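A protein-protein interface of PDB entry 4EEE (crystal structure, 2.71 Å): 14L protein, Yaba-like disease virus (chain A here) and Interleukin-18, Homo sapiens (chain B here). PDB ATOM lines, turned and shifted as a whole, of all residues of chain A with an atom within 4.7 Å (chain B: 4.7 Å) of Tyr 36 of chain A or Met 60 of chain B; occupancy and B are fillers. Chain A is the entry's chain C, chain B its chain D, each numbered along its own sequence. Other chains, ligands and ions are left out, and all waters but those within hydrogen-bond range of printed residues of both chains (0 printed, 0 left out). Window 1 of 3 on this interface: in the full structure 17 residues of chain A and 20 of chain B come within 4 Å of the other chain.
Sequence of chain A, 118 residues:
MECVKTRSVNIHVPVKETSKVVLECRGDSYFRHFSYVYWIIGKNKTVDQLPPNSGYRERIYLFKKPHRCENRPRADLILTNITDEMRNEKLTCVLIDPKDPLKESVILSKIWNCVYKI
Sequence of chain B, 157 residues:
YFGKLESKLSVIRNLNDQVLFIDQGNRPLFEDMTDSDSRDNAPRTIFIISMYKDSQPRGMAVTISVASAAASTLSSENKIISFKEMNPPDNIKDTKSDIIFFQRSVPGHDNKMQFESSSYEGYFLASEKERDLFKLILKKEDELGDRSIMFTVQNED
Of chain B, only Leu 5, Met 51, Tyr 52 and Met 60 come within 4 Å of Tyr 36 of chain A.
Met 60 of chain B touches just these residues of chain A: Phe 34, Tyr 36, Ile 96, Asp 97 and Pro 98.
Of the printed residues of chain B, Asp 97 of chain A touches Met 60 (3.5 Å).
Of the printed residues of chain B, Pro 98 of chain A touches Met 60 (3.7 Å) and Gln 103 (3.4 Å).
Printed residues of chain B within 4 Å of Ile 96 of chain A: Gly 59 and Met 60.
Printed residues of chain A within 4 Å of Met 51 of chain B: Phe 34 and Tyr 36.
Ala 61 of chain B touches none of the printed residues of chain A.
The nearest printed residue of chain A that does not touch Met 60 of chain B is Ser 35 of chain A (5.1 Å).
Of the 11 printed residues of chain B, 7 touch a printed residue of chain A.
Hydrophobic or aromatic side chains of chain B that line the printed part of chain A: Leu 5, Met 51 and Met 60.
Printed residues of chain A that touch a printed residue of chain B: Phe 34, Tyr 36, Tyr 38, Ile 96, Asp 97 and Pro 98.
Hydrophobic or aromatic side chains of chain A that line the printed part of chain B: Phe 34, Tyr 36, Tyr 38, Ile 96 and Pro 98.
Along chain A the printed residues that touch a printed residue of chain B span positions 34 to 98.
Phe 34 of chain A touches Met 51 of chain B.
Tyr 36 of chain A touches Leu 5 of chain B.
Met 51 of chain B touches Tyr 36 of chain A (SD to CE1, 3.5 Å).
CG of Met 60 of chain B touches OH of Tyr 36 of chain A, at 3.4 Å.
Tyr 38 of chain A touches Lys 53 of chain B.
CG2 of Ile 96 of chain A touches O of Gly 59 of chain B, at 3.7 Å.
Ile 96 of chain A touches Met 60 of chain B (CG2 to CA, 3.6 Å).
Asp 97 of chain A touches Met 60 of chain B (O to CB, 3.5 Å).
Pro 98 of chain A touches Met 60 of chain B.
Gln 103 of chain B touches Pro 98 of chain A (O to CA, 3.4 Å).
The side-chain hydroxyl (OH) of Tyr 36 of chain A lies within hydrogen-bond range of the backbone carbonyl oxygen (O) of Tyr 52 of chain B.
The side-chain sulfur (SD) of Met 60 of chain B lies close to the backbone carbonyl oxygen (O) of Phe 34 of chain A.
The backbone carbonyl oxygen (O) of Tyr 36 of chain A sits at hydrogen-bond distance from the backbone NH (N) of Ile 96 of chain A.
N of Val 94 of chain A sits at hydrogen-bond distance from O of Tyr 38 of chain A, 2.9 Å away.
O of Met 51 of chain B is in hydrogen-bond range of N of Leu 5 of chain B.
The backbone NH (N) of Tyr 52 of chain B lies within hydrogen-bond range of the backbone carbonyl oxygen (O) of Ala 61 of chain B (2.7 Å).
O of Met 60 of chain B sits at hydrogen-bond distance from N of Gln 103 of chain B, at 2.9 Å.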
ATOM      1  N   PHE A  34       5.695  24.562 -28.049  1.00  0.00           N
ATOM      2  CA  PHE A  34       6.286  23.236 -27.940  1.00  0.00           C
ATOM      3  C   PHE A  34       7.637  23.116 -28.631  1.00  0.00           C
ATOM      4  O   PHE A  34       7.815  22.305 -29.541  1.00  0.00           O
ATOM      5  CB  PHE A  34       5.332  22.179 -28.493  1.00  0.00           C
ATOM      6  CG  PHE A  34       4.088  22.004 -27.680  1.00  0.00           C
ATOM      7  CD1 PHE A  34       4.108  21.263 -26.511  1.00  0.00           C
ATOM      8  CD2 PHE A  34       2.898  22.588 -28.076  1.00  0.00           C
ATOM      9  CE1 PHE A  34       2.957  21.102 -25.756  1.00  0.00           C
ATOM     10  CE2 PHE A  34       1.745  22.432 -27.328  1.00  0.00           C
ATOM     11  CZ  PHE A  34       1.775  21.689 -26.166  1.00  0.00           C
ATOM     12  N   SER A  35       8.592  23.919 -28.180  1.00  0.00           N
ATOM     13  CA  SER A  35       9.947  23.847 -28.696  1.00  0.00           C
ATOM     14  C   SER A  35      10.947  24.157 -27.587  1.00  0.00           C
ATOM     15  O   SER A  35      10.739  25.063 -26.777  1.00  0.00           O
ATOM     16  CB  SER A  35      10.117  24.795 -29.882  1.00  0.00           C
ATOM     17  OG  SER A  35       9.657  26.105 -29.563  1.00  0.00           O
ATOM     18  N   TYR A  36      12.027  23.385 -27.549  1.00  0.00           N
ATOM     19  CA  TYR A  36      13.063  23.590 -26.550  1.00  0.00           C
ATOM     20  C   TYR A  36      14.384  22.971 -26.989  1.00  0.00           C
ATOM     21  O   TYR A  36      14.413  22.072 -27.837  1.00  0.00           O
ATOM     22  CB  TYR A  36      12.623  23.016 -25.206  1.00  0.00           C
ATOM     23  CG  TYR A  36      12.110  21.605 -25.304  1.00  0.00           C
ATOM     24  CD1 TYR A  36      10.805  21.347 -25.696  1.00  0.00           C
ATOM     25  CD2 TYR A  36      12.931  20.527 -25.019  1.00  0.00           C
ATOM     26  CE1 TYR A  36      10.328  20.051 -25.795  1.00  0.00           C
ATOM     27  CE2 TYR A  36      12.463  19.224 -25.111  1.00  0.00           C
ATOM     28  CZ  TYR A  36      11.158  18.994 -25.500  1.00  0.00           C
ATOM     29  OH  TYR A  36      10.674  17.709 -25.601  1.00  0.00           O
ATOM     30  N   VAL A  37      15.475  23.471 -26.416  1.00  0.00           N
ATOM     31  CA  VAL A  37      16.805  22.952 -26.715  1.00  0.00           C
ATOM     32  C   VAL A  37      17.488  22.449 -25.452  1.00  0.00           C
ATOM     33  O   VAL A  37      17.157  22.868 -24.340  1.00  0.00           O
ATOM     34  CB  VAL A  37      17.700  24.016 -27.352  1.00  0.00           C
ATOM     35  CG1 VAL A  37      17.133  24.440 -28.700  1.00  0.00           C
ATOM     36  CG2 VAL A  37      17.849  25.212 -26.410  1.00  0.00           C
ATOM     37  N   TYR A  38      18.438  21.541 -25.643  1.00  0.00           N
ATOM     38  CA  TYR A  38      19.236  21.002 -24.556  1.00  0.00           C
ATOM     39  C   TYR A  38      20.450  20.272 -25.121  1.00  0.00           C
ATOM     40  O   TYR A  38      20.539  20.031 -26.322  1.00  0.00           O
ATOM     41  CB  TYR A  38      18.405  20.078 -23.663  1.00  0.00           C
ATOM     42  CG  TYR A  38      17.914  18.820 -24.340  1.00  0.00           C
ATOM     43  CD1 TYR A  38      16.811  18.846 -25.182  1.00  0.00           C
ATOM     44  CD2 TYR A  38      18.547  17.604 -24.130  1.00  0.00           C
ATOM     45  CE1 TYR A  38      16.357  17.698 -25.800  1.00  0.00           C
ATOM     46  CE2 TYR A  38      18.100  16.451 -24.744  1.00  0.00           C
ATOM     47  CZ  TYR A  38      17.004  16.504 -25.578  1.00  0.00           C
ATOM     48  OH  TYR A  38      16.555  15.358 -26.190  1.00  0.00           O
ATOM     49  N   PRO A  73      14.186  29.323 -27.818  1.00  0.00           N
ATOM     50  CA  PRO A  73      14.714  28.750 -26.572  1.00  0.00           C
ATOM     51  C   PRO A  73      16.237  28.712 -26.568  1.00  0.00           C
ATOM     52  O   PRO A  73      16.881  28.735 -27.626  1.00  0.00           O
ATOM     53  CB  PRO A  73      14.183  27.314 -26.600  1.00  0.00           C
ATOM     54  CG  PRO A  73      14.133  26.987 -28.064  1.00  0.00           C
ATOM     55  CD  PRO A  73      13.679  28.278 -28.729  1.00  0.00           C
ATOM     56  N   VAL A  94      20.251  19.893 -29.178  1.00  0.00           N
ATOM     57  CA  VAL A  94      19.086  19.363 -29.877  1.00  0.00           C
ATOM     58  C   VAL A  94      17.907  20.316 -29.795  1.00  0.00           C
ATOM     59  O   VAL A  94      17.573  20.822 -28.721  1.00  0.00           O
ATOM     60  CB  VAL A  94      18.642  18.018 -29.296  1.00  0.00           C
ATOM     61  CG1 VAL A  94      17.677  17.338 -30.238  1.00  0.00           C
ATOM     62  CG2 VAL A  94      19.848  17.131 -29.040  1.00  0.00           C
ATOM     63  N   LEU A  95      17.274  20.561 -30.933  1.00  0.00           N
ATOM     64  CA  LEU A  95      15.998  21.249 -30.923  1.00  0.00           C
ATOM     65  C   LEU A  95      14.925  20.173 -30.893  1.00  0.00           C
ATOM     66  O   LEU A  95      14.952  19.245 -31.705  1.00  0.00           O
ATOM     67  CB  LEU A  95      15.845  22.141 -32.152  1.00  0.00           C
ATOM     68  CG  LEU A  95      14.450  22.750 -32.314  1.00  0.00           C
ATOM     69  CD1 LEU A  95      14.056  23.496 -31.038  1.00  0.00           C
ATOM     70  CD2 LEU A  95      14.366  23.652 -33.549  1.00  0.00           C
ATOM     71  N   ILE A  96      14.005  20.282 -29.938  1.00  0.00           N
ATOM     72  CA  ILE A  96      12.852  19.386 -29.881  1.00  0.00           C
ATOM     73  C   ILE A  96      11.544  20.141 -30.072  1.00  0.00           C
ATOM     74  O   ILE A  96      11.214  21.035 -29.287  1.00  0.00           O
ATOM     75  CB  ILE A  96      12.753  18.643 -28.542  1.00  0.00           C
ATOM     76  CG1 ILE A  96      14.025  17.850 -28.280  1.00  0.00           C
ATOM     77  CG2 ILE A  96      11.552  17.714 -28.548  1.00  0.00           C
ATOM     78  CD1 ILE A  96      14.176  16.654 -29.192  1.00  0.00           C
ATOM     79  N   ASP A  97      10.799  19.764 -31.109  1.00  0.00           N
ATOM     80  CA  ASP A  97       9.445  20.267 -31.326  1.00  0.00           C
ATOM     81  C   ASP A  97       8.571  19.131 -31.871  1.00  0.00           C
ATOM     82  O   ASP A  97       9.027  17.988 -31.920  1.00  0.00           O
ATOM     83  CB  ASP A  97       9.447  21.500 -32.244  1.00  0.00           C
ATOM     84  CG  ASP A  97      10.273  21.307 -33.495  1.00  0.00           C
ATOM     85  OD1 ASP A  97      10.717  20.170 -33.760  1.00  0.00           O
ATOM     86  OD2 ASP A  97      10.473  22.312 -34.220  1.00  0.00           O
ATOM     87  N   PRO A  98       7.304  19.424 -32.232  1.00  0.00           N
ATOM     88  CA  PRO A  98       6.443  18.363 -32.782  1.00  0.00           C
ATOM     89  C   PRO A  98       6.892  17.876 -34.163  1.00  0.00           C
ATOM     90  O   PRO A  98       6.148  17.160 -34.833  1.00  0.00           O
ATOM     91  CB  PRO A  98       5.063  19.034 -32.864  1.00  0.00           C
ATOM     92  CG  PRO A  98       5.104  20.090 -31.786  1.00  0.00           C
ATOM     93  CD  PRO A  98       6.521  20.616 -31.848  1.00  0.00           C
ATOM     94  N   LEU B   5      10.715  18.920 -18.369  1.00  0.00           N
ATOM     95  CA  LEU B   5      11.058  20.322 -18.569  1.00  0.00           C
ATOM     96  C   LEU B   5       9.938  21.325 -18.288  1.00  0.00           C
ATOM     97  O   LEU B   5       9.796  21.822 -17.173  1.00  0.00           O
ATOM     98  CB  LEU B   5      11.588  20.542 -19.987  1.00  0.00           C
ATOM     99  CG  LEU B   5      12.946  19.915 -20.308  1.00  0.00           C
ATOM    100  CD1 LEU B   5      13.250  20.021 -21.794  1.00  0.00           C
ATOM    101  CD2 LEU B   5      14.050  20.561 -19.486  1.00  0.00           C
ATOM    102  N   MET B  51       6.560  18.478 -21.385  1.00  0.00           N
ATOM    103  CA  MET B  51       7.645  18.122 -22.290  1.00  0.00           C
ATOM    104  C   MET B  51       8.821  17.535 -21.525  1.00  0.00           C
ATOM    105  O   MET B  51       9.114  17.957 -20.409  1.00  0.00           O
ATOM    106  CB  MET B  51       8.085  19.350 -23.089  1.00  0.00           C
ATOM    107  CG  MET B  51       7.043  19.820 -24.088  1.00  0.00           C
ATOM    108  SD  MET B  51       7.347  21.480 -24.728  1.00  0.00           S
ATOM    109  CE  MET B  51       6.404  22.489 -23.579  1.00  0.00           C
ATOM    110  N   TYR B  52       9.487  16.555 -22.126  1.00  0.00           N
ATOM    111  CA  TYR B  52      10.662  15.942 -21.517  1.00  0.00           C
ATOM    112  C   TYR B  52      11.832  15.959 -22.487  1.00  0.00           C
ATOM    113  O   TYR B  52      11.642  15.829 -23.695  1.00  0.00           O
ATOM    114  CB  TYR B  52      10.364  14.491 -21.123  1.00  0.00           C
ATOM    115  CG  TYR B  52       9.540  14.336 -19.861  1.00  0.00           C
ATOM    116  CD1 TYR B  52       8.217  14.753 -19.809  1.00  0.00           C
ATOM    117  CD2 TYR B  52      10.082  13.745 -18.725  1.00  0.00           C
ATOM    118  CE1 TYR B  52       7.460  14.602 -18.652  1.00  0.00           C
ATOM    119  CE2 TYR B  52       9.333  13.586 -17.564  1.00  0.00           C
ATOM    120  CZ  TYR B  52       8.024  14.016 -17.534  1.00  0.00           C
ATOM    121  OH  TYR B  52       7.276  13.860 -16.384  1.00  0.00           O
ATOM    122  N   LYS B  53      13.040  16.121 -21.958  1.00  0.00           N
ATOM    123  CA  LYS B  53      14.244  15.948 -22.758  1.00  0.00           C
ATOM    124  C   LYS B  53      14.657  14.476 -22.800  1.00  0.00           C
ATOM    125  O   LYS B  53      14.332  13.705 -21.894  1.00  0.00           O
ATOM    126  CB  LYS B  53      15.383  16.784 -22.201  1.00  0.00           C
ATOM    127  CG  LYS B  53      15.870  16.409 -20.825  1.00  0.00           C
ATOM    128  CD  LYS B  53      16.520  17.600 -20.138  1.00  0.00           C
ATOM    129  CE  LYS B  53      17.999  17.392 -19.899  1.00  0.00           C
ATOM    130  NZ  LYS B  53      18.578  18.564 -19.190  1.00  0.00           N
ATOM    131  N   GLY B  59      11.861  12.427 -30.955  1.00  0.00           N
ATOM    132  CA  GLY B  59      10.680  13.254 -31.113  1.00  0.00           C
ATOM    133  C   GLY B  59      10.418  14.008 -29.827  1.00  0.00           C
ATOM    134  O   GLY B  59      11.296  14.074 -28.959  1.00  0.00           O
ATOM    135  N   MET B  60       9.220  14.565 -29.689  1.00  0.00           N
ATOM    136  CA  MET B  60       8.908  15.332 -28.489  1.00  0.00           C
ATOM    137  C   MET B  60       8.226  14.496 -27.405  1.00  0.00           C
ATOM    138  O   MET B  60       7.004  14.313 -27.411  1.00  0.00           O
ATOM    139  CB  MET B  60       8.081  16.573 -28.821  1.00  0.00           C
ATOM    140  CG  MET B  60       7.990  17.543 -27.671  1.00  0.00           C
ATOM    141  SD  MET B  60       7.139  19.056 -28.135  1.00  0.00           S
ATOM    142  CE  MET B  60       5.509  18.398 -28.530  1.00  0.00           C
ATOM    143  N   ALA B  61       9.031  14.000 -26.468  1.00  0.00           N
ATOM    144  CA  ALA B  61       8.530  13.176 -25.366  1.00  0.00           C
ATOM    145  C   ALA B  61       7.679  14.005 -24.413  1.00  0.00           C
ATOM    146  O   ALA B  61       8.154  14.959 -23.799  1.00  0.00           O
ATOM    147  CB  ALA B  61       9.681  12.508 -24.613  1.00  0.00           C
ATOM    148  N   VAL B  62       6.411  13.625 -24.301  1.00  0.00           N
ATOM    149  CA  VAL B  62       5.468  14.333 -23.445  1.00  0.00           C
ATOM    150  C   VAL B  62       4.682  13.372 -22.564  1.00  0.00           C
ATOM    151  O   VAL B  62       4.534  12.191 -22.885  1.00  0.00           O
ATOM    152  CB  VAL B  62       4.461  15.158 -24.263  1.00  0.00           C
ATOM    153  CG1 VAL B  62       5.186  16.073 -25.241  1.00  0.00           C
ATOM    154  CG2 VAL B  62       3.499  14.228 -25.010  1.00  0.00           C
ATOM    155  N   PHE B 101       4.547   9.767 -24.221  1.00  0.00           N
ATOM    156  CA  PHE B 101       4.202   9.708 -25.637  1.00  0.00           C
ATOM    157  C   PHE B 101       5.031  10.690 -26.448  1.00  0.00           C
ATOM    158  O   PHE B 101       5.334  11.794 -25.989  1.00  0.00           O
ATOM    159  CB  PHE B 101       2.711   9.991 -25.842  1.00  0.00           C
ATOM    160  CG  PHE B 101       1.811   9.000 -25.159  1.00  0.00           C
ATOM    161  CD1 PHE B 101       1.519   9.127 -23.806  1.00  0.00           C
ATOM    162  CD2 PHE B 101       1.268   7.933 -25.864  1.00  0.00           C
ATOM    163  CE1 PHE B 101       0.691   8.199 -23.163  1.00  0.00           C
ATOM    164  CE2 PHE B 101       0.438   7.004 -25.229  1.00  0.00           C
ATOM    165  CZ  PHE B 101       0.149   7.137 -23.878  1.00  0.00           C
ATOM    166  N   PHE B 102       5.400  10.276 -27.656  1.00  0.00           N
ATOM    167  CA  PHE B 102       6.017  11.178 -28.617  1.00  0.00           C
ATOM    168  C   PHE B 102       4.929  11.967 -29.332  1.00  0.00           C
ATOM    169  O   PHE B 102       4.043  11.385 -29.977  1.00  0.00           O
ATOM    170  CB  PHE B 102       6.859  10.397 -29.627  1.00  0.00           C
ATOM    171  CG  PHE B 102       7.972   9.614 -28.994  1.00  0.00           C
ATOM    172  CD1 PHE B 102       9.100  10.254 -28.497  1.00  0.00           C
ATOM    173  CD2 PHE B 102       7.886   8.236 -28.880  1.00  0.00           C
ATOM    174  CE1 PHE B 102      10.125   9.526 -27.903  1.00  0.00           C
ATOM    175  CE2 PHE B 102       8.907   7.505 -28.292  1.00  0.00           C
ATOM    176  CZ  PHE B 102      10.025   8.152 -27.803  1.00  0.00           C
ATOM    177  N   GLN B 103       4.984  13.290 -29.195  1.00  0.00           N
ATOM    178  CA  GLN B 103       3.986  14.166 -29.811  1.00  0.00           C
ATOM    179  C   GLN B 103       4.502  14.662 -31.146  1.00  0.00           C
ATOM    180  O   GLN B 103       5.365  15.542 -31.206  1.00  0.00           O
ATOM    181  CB  GLN B 103       3.648  15.347 -28.905  1.00  0.00           C
ATOM    182  CG  GLN B 103       2.701  16.338 -29.543  1.00  0.00           C
ATOM    183  CD  GLN B 103       2.337  17.459 -28.604  1.00  0.00           C
ATOM    184  OE1 GLN B 103       2.293  17.263 -27.386  1.00  0.00           O
ATOM    185  NE2 GLN B 103       2.085  18.651 -29.160  1.00  0.00           N
